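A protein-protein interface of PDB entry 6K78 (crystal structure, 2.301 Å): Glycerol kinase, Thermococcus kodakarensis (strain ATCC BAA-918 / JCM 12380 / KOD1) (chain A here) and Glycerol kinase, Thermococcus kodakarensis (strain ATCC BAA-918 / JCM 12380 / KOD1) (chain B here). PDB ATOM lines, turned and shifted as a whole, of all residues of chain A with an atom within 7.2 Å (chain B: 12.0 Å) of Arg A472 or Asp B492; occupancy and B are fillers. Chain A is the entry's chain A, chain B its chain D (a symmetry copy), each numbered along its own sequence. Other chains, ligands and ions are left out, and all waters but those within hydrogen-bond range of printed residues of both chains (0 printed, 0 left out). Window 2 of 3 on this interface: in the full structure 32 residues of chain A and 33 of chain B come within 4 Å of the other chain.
Of the 10 printed residues of chain B, 5 touch a printed residue of chain A.
Hydrophobic or aromatic side chains of chain B that line the printed part of chain A: Trp B487, Val B490 and Val B491.
Printed residues of chain A that touch a printed residue of chain B: Glu A333, Gly A334, Tyr A336, Arg A472 and Gly A476.
Hydrophobic or aromatic side chains of chain A within 4 Å of the printed part of chain B: Tyr A336.
Among the printed residues, no Asp or Glu carboxylate lies within 4 Å of a Lys or Arg side-chain nitrogen of the other chain.
The indole nitrogen (NE1) of Trp B487 lies within hydrogen-bond range of the backbone carbonyl oxygen (O) of Gly A334 (3.0 Å).
Among the printed residues, pairs that only touch across the chains: Glu A333 with Ser B493, Gly A334 with Val B491, Tyr A336 with Trp B487, Arg A472 with Asp B492, Gly A476 with Trp B487 and Gly A476 with Val B490.
Of chain A, only Arg A472 (3.6 Å) comes within 4 Å of Asp B492.
Of the printed residues of chain B, Gly A334 touches Trp B487 and Val B491.
No residue of chain B comes within 4 Å of Lys A468.
No residue of chain B comes within 4 Å of Thr A469.
No residue of chain B comes within 4 Å of Leu A473.
No residue of chain B comes within 4 Å of Lys A475.
Gly A476 touches just these residues of chain B: Trp B487 (3.4 Å) and Val B490 (3.7 Å).
Printed residues of chain A within 4 Å of Ser B493: Glu A333 (3.9 Å).
Of the printed residues of chain A, Val B491 touches Gly A334.
The nearest residue of chain A that does not touch Asp B492 is Gly A334 (5.5 Å).
The backbone NH (N) of Glu A333 is in hydrogen-bond range of the side-chain hydroxyl (OG) of Ser A331.
The backbone NH (N) of Gly A334 lies within hydrogen-bond range of the side-chain amide oxygen (OD1) of Asn A332.
The side-chain hydroxyl (OH) of Tyr A336 sits close to the side-chain amide nitrogen (ND2) of Asn A332, at 3.2 Å.
OH of Tyr A336 is in hydrogen-bond range of O of Leu A473, 2.9 Å away.
N of Trp B487 is in hydrogen-bond range of O of Phe B352, 3.3 Å away.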
ATOM      1  N   SER A 331      23.739  18.551 -17.452  1.00  0.00           N
ATOM      2  CA  SER A 331      22.798  19.657 -17.272  1.00  0.00           C
ATOM      3  C   SER A 331      22.902  20.162 -15.833  1.00  0.00           C
ATOM      4  O   SER A 331      23.663  19.633 -15.026  1.00  0.00           O
ATOM      5  CB  SER A 331      21.365  19.234 -17.600  1.00  0.00           C
ATOM      6  OG  SER A 331      20.689  18.781 -16.434  1.00  0.00           O
ATOM      7  N   ASN A 332      22.103  21.176 -15.506  1.00  0.00           N
ATOM      8  CA  ASN A 332      22.162  21.718 -14.159  1.00  0.00           C
ATOM      9  C   ASN A 332      21.364  20.879 -13.157  1.00  0.00           C
ATOM     10  O   ASN A 332      21.395  21.179 -11.954  1.00  0.00           O
ATOM     11  CB  ASN A 332      21.719  23.199 -14.156  1.00  0.00           C
ATOM     12  CG  ASN A 332      20.258  23.396 -14.559  1.00  0.00           C
ATOM     13  OD1 ASN A 332      19.426  22.516 -14.386  1.00  0.00           O
ATOM     14  ND2 ASN A 332      19.950  24.573 -15.100  1.00  0.00           N
ATOM     15  N   GLU A 333      20.679  19.834 -13.636  1.00  0.00           N
ATOM     16  CA  GLU A 333      19.910  18.891 -12.810  1.00  0.00           C
ATOM     17  C   GLU A 333      18.970  19.605 -11.839  1.00  0.00           C
ATOM     18  O   GLU A 333      18.680  19.096 -10.752  1.00  0.00           O
ATOM     19  CB  GLU A 333      20.836  17.920 -12.059  1.00  0.00           C
ATOM     20  CG  GLU A 333      21.921  17.343 -12.963  1.00  0.00           C
ATOM     21  CD  GLU A 333      22.541  16.047 -12.473  1.00  0.00           C
ATOM     22  OE1 GLU A 333      22.972  15.965 -11.304  1.00  0.00           O
ATOM     23  OE2 GLU A 333      22.644  15.109 -13.288  1.00  0.00           O
ATOM     24  N   GLY A 334      18.477  20.783 -12.237  1.00  0.00           N
ATOM     25  CA  GLY A 334      17.538  21.560 -11.448  1.00  0.00           C
ATOM     26  C   GLY A 334      18.160  22.520 -10.462  1.00  0.00           C
ATOM     27  O   GLY A 334      17.418  23.195  -9.729  1.00  0.00           O
ATOM     28  N   TYR A 336      19.939  25.924  -9.511  1.00  0.00           N
ATOM     29  CA  TYR A 336      20.141  27.290  -9.950  1.00  0.00           C
ATOM     30  C   TYR A 336      20.725  28.089  -8.795  1.00  0.00           C
ATOM     31  O   TYR A 336      20.544  27.752  -7.622  1.00  0.00           O
ATOM     32  CB  TYR A 336      18.824  27.931 -10.437  1.00  0.00           C
ATOM     33  CG  TYR A 336      18.371  27.449 -11.807  1.00  0.00           C
ATOM     34  CD1 TYR A 336      17.904  26.142 -11.991  1.00  0.00           C
ATOM     35  CD2 TYR A 336      18.436  28.282 -12.923  1.00  0.00           C
ATOM     36  CE1 TYR A 336      17.499  25.687 -13.239  1.00  0.00           C
ATOM     37  CE2 TYR A 336      18.032  27.824 -14.187  1.00  0.00           C
ATOM     38  CZ  TYR A 336      17.564  26.543 -14.330  1.00  0.00           C
ATOM     39  OH  TYR A 336      17.165  26.088 -15.557  1.00  0.00           O
ATOM     40  N   TYR A 379      22.884  33.682 -17.735  1.00  0.00           N
ATOM     41  CA  TYR A 379      21.487  34.112 -17.638  1.00  0.00           C
ATOM     42  C   TYR A 379      21.390  35.618 -17.404  1.00  0.00           C
ATOM     43  O   TYR A 379      20.622  36.310 -18.075  1.00  0.00           O
ATOM     44  CB  TYR A 379      20.763  33.368 -16.506  1.00  0.00           C
ATOM     45  CG  TYR A 379      20.579  31.881 -16.683  1.00  0.00           C
ATOM     46  CD1 TYR A 379      20.075  31.351 -17.864  1.00  0.00           C
ATOM     47  CD2 TYR A 379      20.885  31.011 -15.654  1.00  0.00           C
ATOM     48  CE1 TYR A 379      19.883  29.968 -18.026  1.00  0.00           C
ATOM     49  CE2 TYR A 379      20.717  29.655 -15.792  1.00  0.00           C
ATOM     50  CZ  TYR A 379      20.213  29.127 -16.974  1.00  0.00           C
ATOM     51  OH  TYR A 379      20.053  27.764 -17.083  1.00  0.00           O
ATOM     52  N   ILE A 416      22.392  29.672 -24.789  1.00  0.00           N
ATOM     53  CA  ILE A 416      21.231  30.273 -24.141  1.00  0.00           C
ATOM     54  C   ILE A 416      20.774  31.539 -24.845  1.00  0.00           C
ATOM     55  O   ILE A 416      19.618  31.936 -24.686  1.00  0.00           O
ATOM     56  CB  ILE A 416      21.543  30.564 -22.654  1.00  0.00           C
ATOM     57  CG1 ILE A 416      20.286  30.431 -21.791  1.00  0.00           C
ATOM     58  CG2 ILE A 416      22.071  31.950 -22.474  1.00  0.00           C
ATOM     59  CD1 ILE A 416      19.716  29.031 -21.760  1.00  0.00           C
ATOM     60  N   ASP A 466      18.806  23.595 -28.885  1.00  0.00           N
ATOM     61  CA  ASP A 466      17.526  23.843 -29.537  1.00  0.00           C
ATOM     62  C   ASP A 466      16.663  24.789 -28.689  1.00  0.00           C
ATOM     63  O   ASP A 466      16.915  25.030 -27.503  1.00  0.00           O
ATOM     64  CB  ASP A 466      16.792  22.524 -29.831  1.00  0.00           C
ATOM     65  CG  ASP A 466      16.384  21.747 -28.559  1.00  0.00           C
ATOM     66  OD1 ASP A 466      15.931  22.357 -27.569  1.00  0.00           O
ATOM     67  OD2 ASP A 466      16.479  20.500 -28.558  1.00  0.00           O
ATOM     68  N   GLU A 467      15.614  25.318 -29.322  1.00  0.00           N
ATOM     69  CA  GLU A 467      14.776  26.334 -28.689  1.00  0.00           C
ATOM     70  C   GLU A 467      14.038  25.799 -27.460  1.00  0.00           C
ATOM     71  O   GLU A 467      13.839  26.527 -26.481  1.00  0.00           O
ATOM     72  CB  GLU A 467      13.784  26.870 -29.721  1.00  0.00           C
ATOM     73  CG  GLU A 467      13.119  28.181 -29.343  1.00  0.00           C
ATOM     74  CD  GLU A 467      14.084  29.352 -29.321  1.00  0.00           C
ATOM     75  OE1 GLU A 467      15.218  29.223 -29.845  1.00  0.00           O
ATOM     76  OE2 GLU A 467      13.694  30.419 -28.797  1.00  0.00           O
ATOM     77  N   LYS A 468      13.605  24.541 -27.497  1.00  0.00           N
ATOM     78  CA  LYS A 468      12.921  23.968 -26.341  1.00  0.00           C
ATOM     79  C   LYS A 468      13.806  24.031 -25.095  1.00  0.00           C
ATOM     80  O   LYS A 468      13.375  24.499 -24.033  1.00  0.00           O
ATOM     81  CB  LYS A 468      12.502  22.525 -26.646  1.00  0.00           C
ATOM     82  CG  LYS A 468      12.121  21.711 -25.419  1.00  0.00           C
ATOM     83  CD  LYS A 468      11.511  20.375 -25.794  1.00  0.00           C
ATOM     84  CE  LYS A 468      12.101  19.809 -27.087  1.00  0.00           C
ATOM     85  NZ  LYS A 468      13.273  18.902 -26.849  1.00  0.00           N
ATOM     86  N   THR A 469      15.065  23.596 -25.225  1.00  0.00           N
ATOM     87  CA  THR A 469      15.989  23.594 -24.092  1.00  0.00           C
ATOM     88  C   THR A 469      16.297  25.010 -23.601  1.00  0.00           C
ATOM     89  O   THR A 469      16.207  25.292 -22.402  1.00  0.00           O
ATOM     90  CB  THR A 469      17.263  22.867 -24.490  1.00  0.00           C
ATOM     91  OG1 THR A 469      16.911  21.546 -24.936  1.00  0.00           O
ATOM     92  CG2 THR A 469      18.223  22.790 -23.306  1.00  0.00           C
ATOM     93  N   ARG A 470      16.661  25.911 -24.520  1.00  0.00           N
ATOM     94  CA  ARG A 470      16.900  27.313 -24.199  1.00  0.00           C
ATOM     95  C   ARG A 470      15.795  27.887 -23.319  1.00  0.00           C
ATOM     96  O   ARG A 470      16.060  28.507 -22.280  1.00  0.00           O
ATOM     97  CB  ARG A 470      17.014  28.110 -25.511  1.00  0.00           C
ATOM     98  CG  ARG A 470      18.090  29.182 -25.583  1.00  0.00           C
ATOM     99  CD  ARG A 470      17.938  30.182 -26.780  1.00  0.00           C
ATOM    100  NE  ARG A 470      17.360  29.609 -28.004  1.00  0.00           N
ATOM    101  CZ  ARG A 470      17.941  28.676 -28.758  1.00  0.00           C
ATOM    102  NH1 ARG A 470      19.134  28.199 -28.418  1.00  0.00           N
ATOM    103  NH2 ARG A 470      17.326  28.215 -29.846  1.00  0.00           N
ATOM    104  N   GLU A 471      14.542  27.717 -23.741  1.00  0.00           N
ATOM    105  CA  GLU A 471      13.447  28.348 -23.013  1.00  0.00           C
ATOM    106  C   GLU A 471      13.153  27.617 -21.711  1.00  0.00           C
ATOM    107  O   GLU A 471      12.794  28.252 -20.716  1.00  0.00           O
ATOM    108  CB  GLU A 471      12.202  28.439 -23.902  1.00  0.00           C
ATOM    109  CG  GLU A 471      12.357  29.465 -25.042  1.00  0.00           C
ATOM    110  CD  GLU A 471      12.919  30.810 -24.553  1.00  0.00           C
ATOM    111  OE1 GLU A 471      12.164  31.540 -23.868  1.00  0.00           O
ATOM    112  OE2 GLU A 471      14.111  31.139 -24.836  1.00  0.00           O
ATOM    113  N   ARG A 472      13.343  26.300 -21.672  1.00  0.00           N
ATOM    114  CA  ARG A 472      13.215  25.605 -20.399  1.00  0.00           C
ATOM    115  C   ARG A 472      14.246  26.117 -19.392  1.00  0.00           C
ATOM    116  O   ARG A 472      13.901  26.442 -18.248  1.00  0.00           O
ATOM    117  CB  ARG A 472      13.343  24.094 -20.598  1.00  0.00           C
ATOM    118  CG  ARG A 472      13.049  23.305 -19.333  1.00  0.00           C
ATOM    119  CD  ARG A 472      12.876  21.822 -19.599  1.00  0.00           C
ATOM    120  NE  ARG A 472      13.871  21.282 -20.531  1.00  0.00           N
ATOM    121  CZ  ARG A 472      15.115  20.940 -20.201  1.00  0.00           C
ATOM    122  NH1 ARG A 472      15.549  21.088 -18.947  1.00  0.00           N
ATOM    123  NH2 ARG A 472      15.935  20.456 -21.125  1.00  0.00           N
ATOM    124  N   LEU A 473      15.516  26.232 -19.813  1.00  0.00           N
ATOM    125  CA  LEU A 473      16.569  26.594 -18.867  1.00  0.00           C
ATOM    126  C   LEU A 473      16.439  28.044 -18.436  1.00  0.00           C
ATOM    127  O   LEU A 473      16.682  28.377 -17.274  1.00  0.00           O
ATOM    128  CB  LEU A 473      17.950  26.330 -19.474  1.00  0.00           C
ATOM    129  CG  LEU A 473      18.248  24.853 -19.689  1.00  0.00           C
ATOM    130  CD1 LEU A 473      19.618  24.639 -20.309  1.00  0.00           C
ATOM    131  CD2 LEU A 473      18.107  24.138 -18.365  1.00  0.00           C
ATOM    132  N   TYR A 474      16.060  28.920 -19.363  1.00  0.00           N
ATOM    133  CA  TYR A 474      15.788  30.301 -19.003  1.00  0.00           C
ATOM    134  C   TYR A 474      14.566  30.403 -18.099  1.00  0.00           C
ATOM    135  O   TYR A 474      14.512  31.285 -17.229  1.00  0.00           O
ATOM    136  CB  TYR A 474      15.593  31.142 -20.269  1.00  0.00           C
ATOM    137  CG  TYR A 474      15.811  32.614 -20.057  1.00  0.00           C
ATOM    138  CD1 TYR A 474      16.913  33.078 -19.326  1.00  0.00           C
ATOM    139  CD2 TYR A 474      14.928  33.552 -20.589  1.00  0.00           C
ATOM    140  CE1 TYR A 474      17.116  34.434 -19.123  1.00  0.00           C
ATOM    141  CE2 TYR A 474      15.125  34.913 -20.396  1.00  0.00           C
ATOM    142  CZ  TYR A 474      16.225  35.344 -19.659  1.00  0.00           C
ATOM    143  OH  TYR A 474      16.440  36.678 -19.431  1.00  0.00           O
ATOM    144  N   LYS A 475      13.587  29.510 -18.286  1.00  0.00           N
ATOM    145  CA  LYS A 475      12.385  29.534 -17.456  1.00  0.00           C
ATOM    146  C   LYS A 475      12.718  29.199 -16.002  1.00  0.00           C
ATOM    147  O   LYS A 475      12.238  29.859 -15.075  1.00  0.00           O
ATOM    148  CB  LYS A 475      11.336  28.559 -18.001  1.00  0.00           C
ATOM    149  CG  LYS A 475      10.105  28.424 -17.110  1.00  0.00           C
ATOM    150  CD  LYS A 475       9.235  29.685 -17.145  1.00  0.00           C
ATOM    151  CE  LYS A 475       7.746  29.356 -17.330  1.00  0.00           C
ATOM    152  NZ  LYS A 475       7.468  28.745 -18.676  1.00  0.00           N
ATOM    153  N   GLY A 476      13.559  28.184 -15.783  1.00  0.00           N
ATOM    154  CA  GLY A 476      14.042  27.908 -14.432  1.00  0.00           C
ATOM    155  C   GLY A 476      14.767  29.099 -13.847  1.00  0.00           C
ATOM    156  O   GLY A 476      14.605  29.428 -12.666  1.00  0.00           O
ATOM    157  N   TRP A 477      15.529  29.800 -14.685  1.00  0.00           N
ATOM    158  CA  TRP A 477      16.236  30.975 -14.207  1.00  0.00           C
ATOM    159  C   TRP A 477      15.253  32.035 -13.752  1.00  0.00           C
ATOM    160  O   TRP A 477      15.451  32.688 -12.715  1.00  0.00           O
ATOM    161  CB  TRP A 477      17.147  31.522 -15.305  1.00  0.00           C
ATOM    162  CG  TRP A 477      17.628  32.891 -15.013  1.00  0.00           C
ATOM    163  CD1 TRP A 477      17.210  34.048 -15.594  1.00  0.00           C
ATOM    164  CD2 TRP A 477      18.612  33.258 -14.045  1.00  0.00           C
ATOM    165  NE1 TRP A 477      17.888  35.123 -15.048  1.00  0.00           N
ATOM    166  CE2 TRP A 477      18.756  34.657 -14.100  1.00  0.00           C
ATOM    167  CE3 TRP A 477      19.403  32.537 -13.152  1.00  0.00           C
ATOM    168  CZ2 TRP A 477      19.657  35.341 -13.299  1.00  0.00           C
ATOM    169  CZ3 TRP A 477      20.290  33.227 -12.358  1.00  0.00           C
ATOM    170  CH2 TRP A 477      20.410  34.603 -12.437  1.00  0.00           C
ATOM    171  N   LYS A 478      14.171  32.204 -14.511  1.00  0.00           N
ATOM    172  CA  LYS A 478      13.196  33.232 -14.180  1.00  0.00           C
ATOM    173  C   LYS A 478      12.460  32.882 -12.892  1.00  0.00           C
ATOM    174  O   LYS A 478      12.271  33.742 -12.024  1.00  0.00           O
ATOM    175  CB  LYS A 478      12.242  33.426 -15.358  1.00  0.00           C
ATOM    176  CG  LYS A 478      12.901  34.186 -16.497  1.00  0.00           C
ATOM    177  CD  LYS A 478      11.906  34.784 -17.480  1.00  0.00           C
ATOM    178  CE  LYS A 478      11.043  33.708 -18.120  1.00  0.00           C
ATOM    179  NZ  LYS A 478      10.113  34.293 -19.146  1.00  0.00           N
ATOM    180  N   PHE B 352       7.263  18.168  -3.930  1.00  0.00           N
ATOM    181  CA  PHE B 352       8.040  18.731  -5.019  1.00  0.00           C
ATOM    182  C   PHE B 352       8.912  19.891  -4.575  1.00  0.00           C
ATOM    183  O   PHE B 352       9.686  20.408  -5.393  1.00  0.00           O
ATOM    184  CB  PHE B 352       7.117  19.172  -6.171  1.00  0.00           C
ATOM    185  CG  PHE B 352       6.367  18.029  -6.793  1.00  0.00           C
ATOM    186  CD1 PHE B 352       7.065  16.957  -7.355  1.00  0.00           C
ATOM    187  CD2 PHE B 352       4.972  17.986  -6.760  1.00  0.00           C
ATOM    188  CE1 PHE B 352       6.382  15.869  -7.903  1.00  0.00           C
ATOM    189  CE2 PHE B 352       4.283  16.902  -7.306  1.00  0.00           C
ATOM    190  CZ  PHE B 352       4.990  15.840  -7.877  1.00  0.00           C
ATOM    191  N   ARG B 354      12.164  21.576  -3.040  1.00  0.00           N
ATOM    192  CA  ARG B 354      13.547  21.141  -3.120  1.00  0.00           C
ATOM    193  C   ARG B 354      14.351  22.074  -2.235  1.00  0.00           C
ATOM    194  O   ARG B 354      13.817  23.042  -1.686  1.00  0.00           O
ATOM    195  CB  ARG B 354      14.050  21.113  -4.571  1.00  0.00           C
ATOM    196  CG  ARG B 354      13.404  20.027  -5.437  1.00  0.00           C
ATOM    197  CD  ARG B 354      13.900  18.674  -5.002  1.00  0.00           C
ATOM    198  NE  ARG B 354      13.273  17.550  -5.695  1.00  0.00           N
ATOM    199  CZ  ARG B 354      12.060  17.075  -5.410  1.00  0.00           C
ATOM    200  NH1 ARG B 354      11.321  17.633  -4.454  1.00  0.00           N
ATOM    201  NH2 ARG B 354      11.584  16.036  -6.076  1.00  0.00           N
ATOM    202  N   GLY B 486       7.226  23.595  -4.392  1.00  0.00           N
ATOM    203  CA  GLY B 486       6.946  23.112  -5.735  1.00  0.00           C
ATOM    204  C   GLY B 486       8.057  23.292  -6.750  1.00  0.00           C
ATOM    205  O   GLY B 486       7.801  23.194  -7.953  1.00  0.00           O
ATOM    206  N   TRP B 487       9.301  23.512  -6.301  1.00  0.00           N
ATOM    207  CA  TRP B 487      10.380  23.865  -7.223  1.00  0.00           C
ATOM    208  C   TRP B 487      10.558  22.838  -8.336  1.00  0.00           C
ATOM    209  O   TRP B 487      10.951  23.206  -9.446  1.00  0.00           O
ATOM    210  CB  TRP B 487      11.703  24.032  -6.480  1.00  0.00           C
ATOM    211  CG  TRP B 487      12.840  24.235  -7.444  1.00  0.00           C
ATOM    212  CD1 TRP B 487      13.866  23.361  -7.722  1.00  0.00           C
ATOM    213  CD2 TRP B 487      13.031  25.362  -8.304  1.00  0.00           C
ATOM    214  NE1 TRP B 487      14.690  23.895  -8.677  1.00  0.00           N
ATOM    215  CE2 TRP B 487      14.205  25.123  -9.050  1.00  0.00           C
ATOM    216  CE3 TRP B 487      12.332  26.560  -8.507  1.00  0.00           C
ATOM    217  CZ2 TRP B 487      14.696  26.043  -9.981  1.00  0.00           C
ATOM    218  CZ3 TRP B 487      12.825  27.472  -9.426  1.00  0.00           C
ATOM    219  CH2 TRP B 487      13.990  27.203 -10.158  1.00  0.00           C
ATOM    220  N   ALA B 488      10.284  21.566  -8.068  1.00  0.00           N
ATOM    221  CA  ALA B 488      10.391  20.542  -9.096  1.00  0.00           C
ATOM    222  C   ALA B 488       9.209  20.546 -10.067  1.00  0.00           C
ATOM    223  O   ALA B 488       9.156  19.682 -10.954  1.00  0.00           O
ATOM    224  CB  ALA B 488      10.539  19.165  -8.454  1.00  0.00           C
ATOM    225  N   LYS B 489       8.250  21.470  -9.901  1.00  0.00           N
ATOM    226  CA  LYS B 489       7.340  21.801 -11.001  1.00  0.00           C
ATOM    227  C   LYS B 489       8.051  22.634 -12.057  1.00  0.00           C
ATOM    228  O   LYS B 489       7.765  22.508 -13.252  1.00  0.00           O
ATOM    229  CB  LYS B 489       6.110  22.571 -10.497  1.00  0.00           C
ATOM    230  CG  LYS B 489       5.305  21.875  -9.420  1.00  0.00           C
ATOM    231  CD  LYS B 489       4.054  22.663  -9.112  1.00  0.00           C
ATOM    232  CE  LYS B 489       2.819  21.961  -9.676  1.00  0.00           C
ATOM    233  NZ  LYS B 489       2.554  20.665  -8.981  1.00  0.00           N
ATOM    234  N   VAL B 490       8.980  23.494 -11.630  1.00  0.00           N
ATOM    235  CA  VAL B 490       9.623  24.439 -12.534  1.00  0.00           C
ATOM    236  C   VAL B 490      10.621  23.740 -13.450  1.00  0.00           C
ATOM    237  O   VAL B 490      10.666  24.012 -14.654  1.00  0.00           O
ATOM    238  CB  VAL B 490      10.302  25.552 -11.724  1.00  0.00           C
ATOM    239  CG1 VAL B 490      11.264  26.324 -12.611  1.00  0.00           C
ATOM    240  CG2 VAL B 490       9.263  26.470 -11.096  1.00  0.00           C
ATOM    241  N   VAL B 491      11.443  22.848 -12.906  1.00  0.00           N
ATOM    242  CA  VAL B 491      12.575  22.295 -13.640  1.00  0.00           C
ATOM    243  C   VAL B 491      12.296  20.853 -14.026  1.00  0.00           C
ATOM    244  O   VAL B 491      11.407  20.193 -13.488  1.00  0.00           O
ATOM    245  CB  VAL B 491      13.893  22.385 -12.845  1.00  0.00           C
ATOM    246  CG1 VAL B 491      14.082  23.792 -12.313  1.00  0.00           C
ATOM    247  CG2 VAL B 491      13.914  21.350 -11.716  1.00  0.00           C
ATOM    248  N   ASP B 492      13.077  20.369 -14.988  1.00  0.00           N
ATOM    249  CA  ASP B 492      13.022  18.995 -15.470  1.00  0.00           C
ATOM    250  C   ASP B 492      14.310  18.321 -15.006  1.00  0.00           C
ATOM    251  O   ASP B 492      15.248  18.123 -15.784  1.00  0.00           O
ATOM    252  CB  ASP B 492      12.862  18.948 -17.039  1.00  0.00           C
ATOM    253  CG  ASP B 492      11.397  18.971 -17.492  1.00  0.00           C
ATOM    254  OD1 ASP B 492      10.505  19.156 -16.626  1.00  0.00           O
ATOM    255  OD2 ASP B 492      11.135  18.798 -18.713  1.00  0.00           O
ATOM    256  N   SER B 493      14.349  17.968 -13.721  1.00  0.00           N
ATOM    257  CA  SER B 493      15.559  17.454 -13.063  1.00  0.00           C
ATOM    258  C   SER B 493      16.152  16.200 -13.711  1.00  0.00           C
ATOM    259  O   SER B 493      17.352  15.927 -13.575  1.00  0.00           O
ATOM    260  CB  SER B 493      15.262  17.164 -11.591  1.00  0.00           C
ATOM    261  OG  SER B 493      16.123  16.157 -11.082  1.00  0.00           O
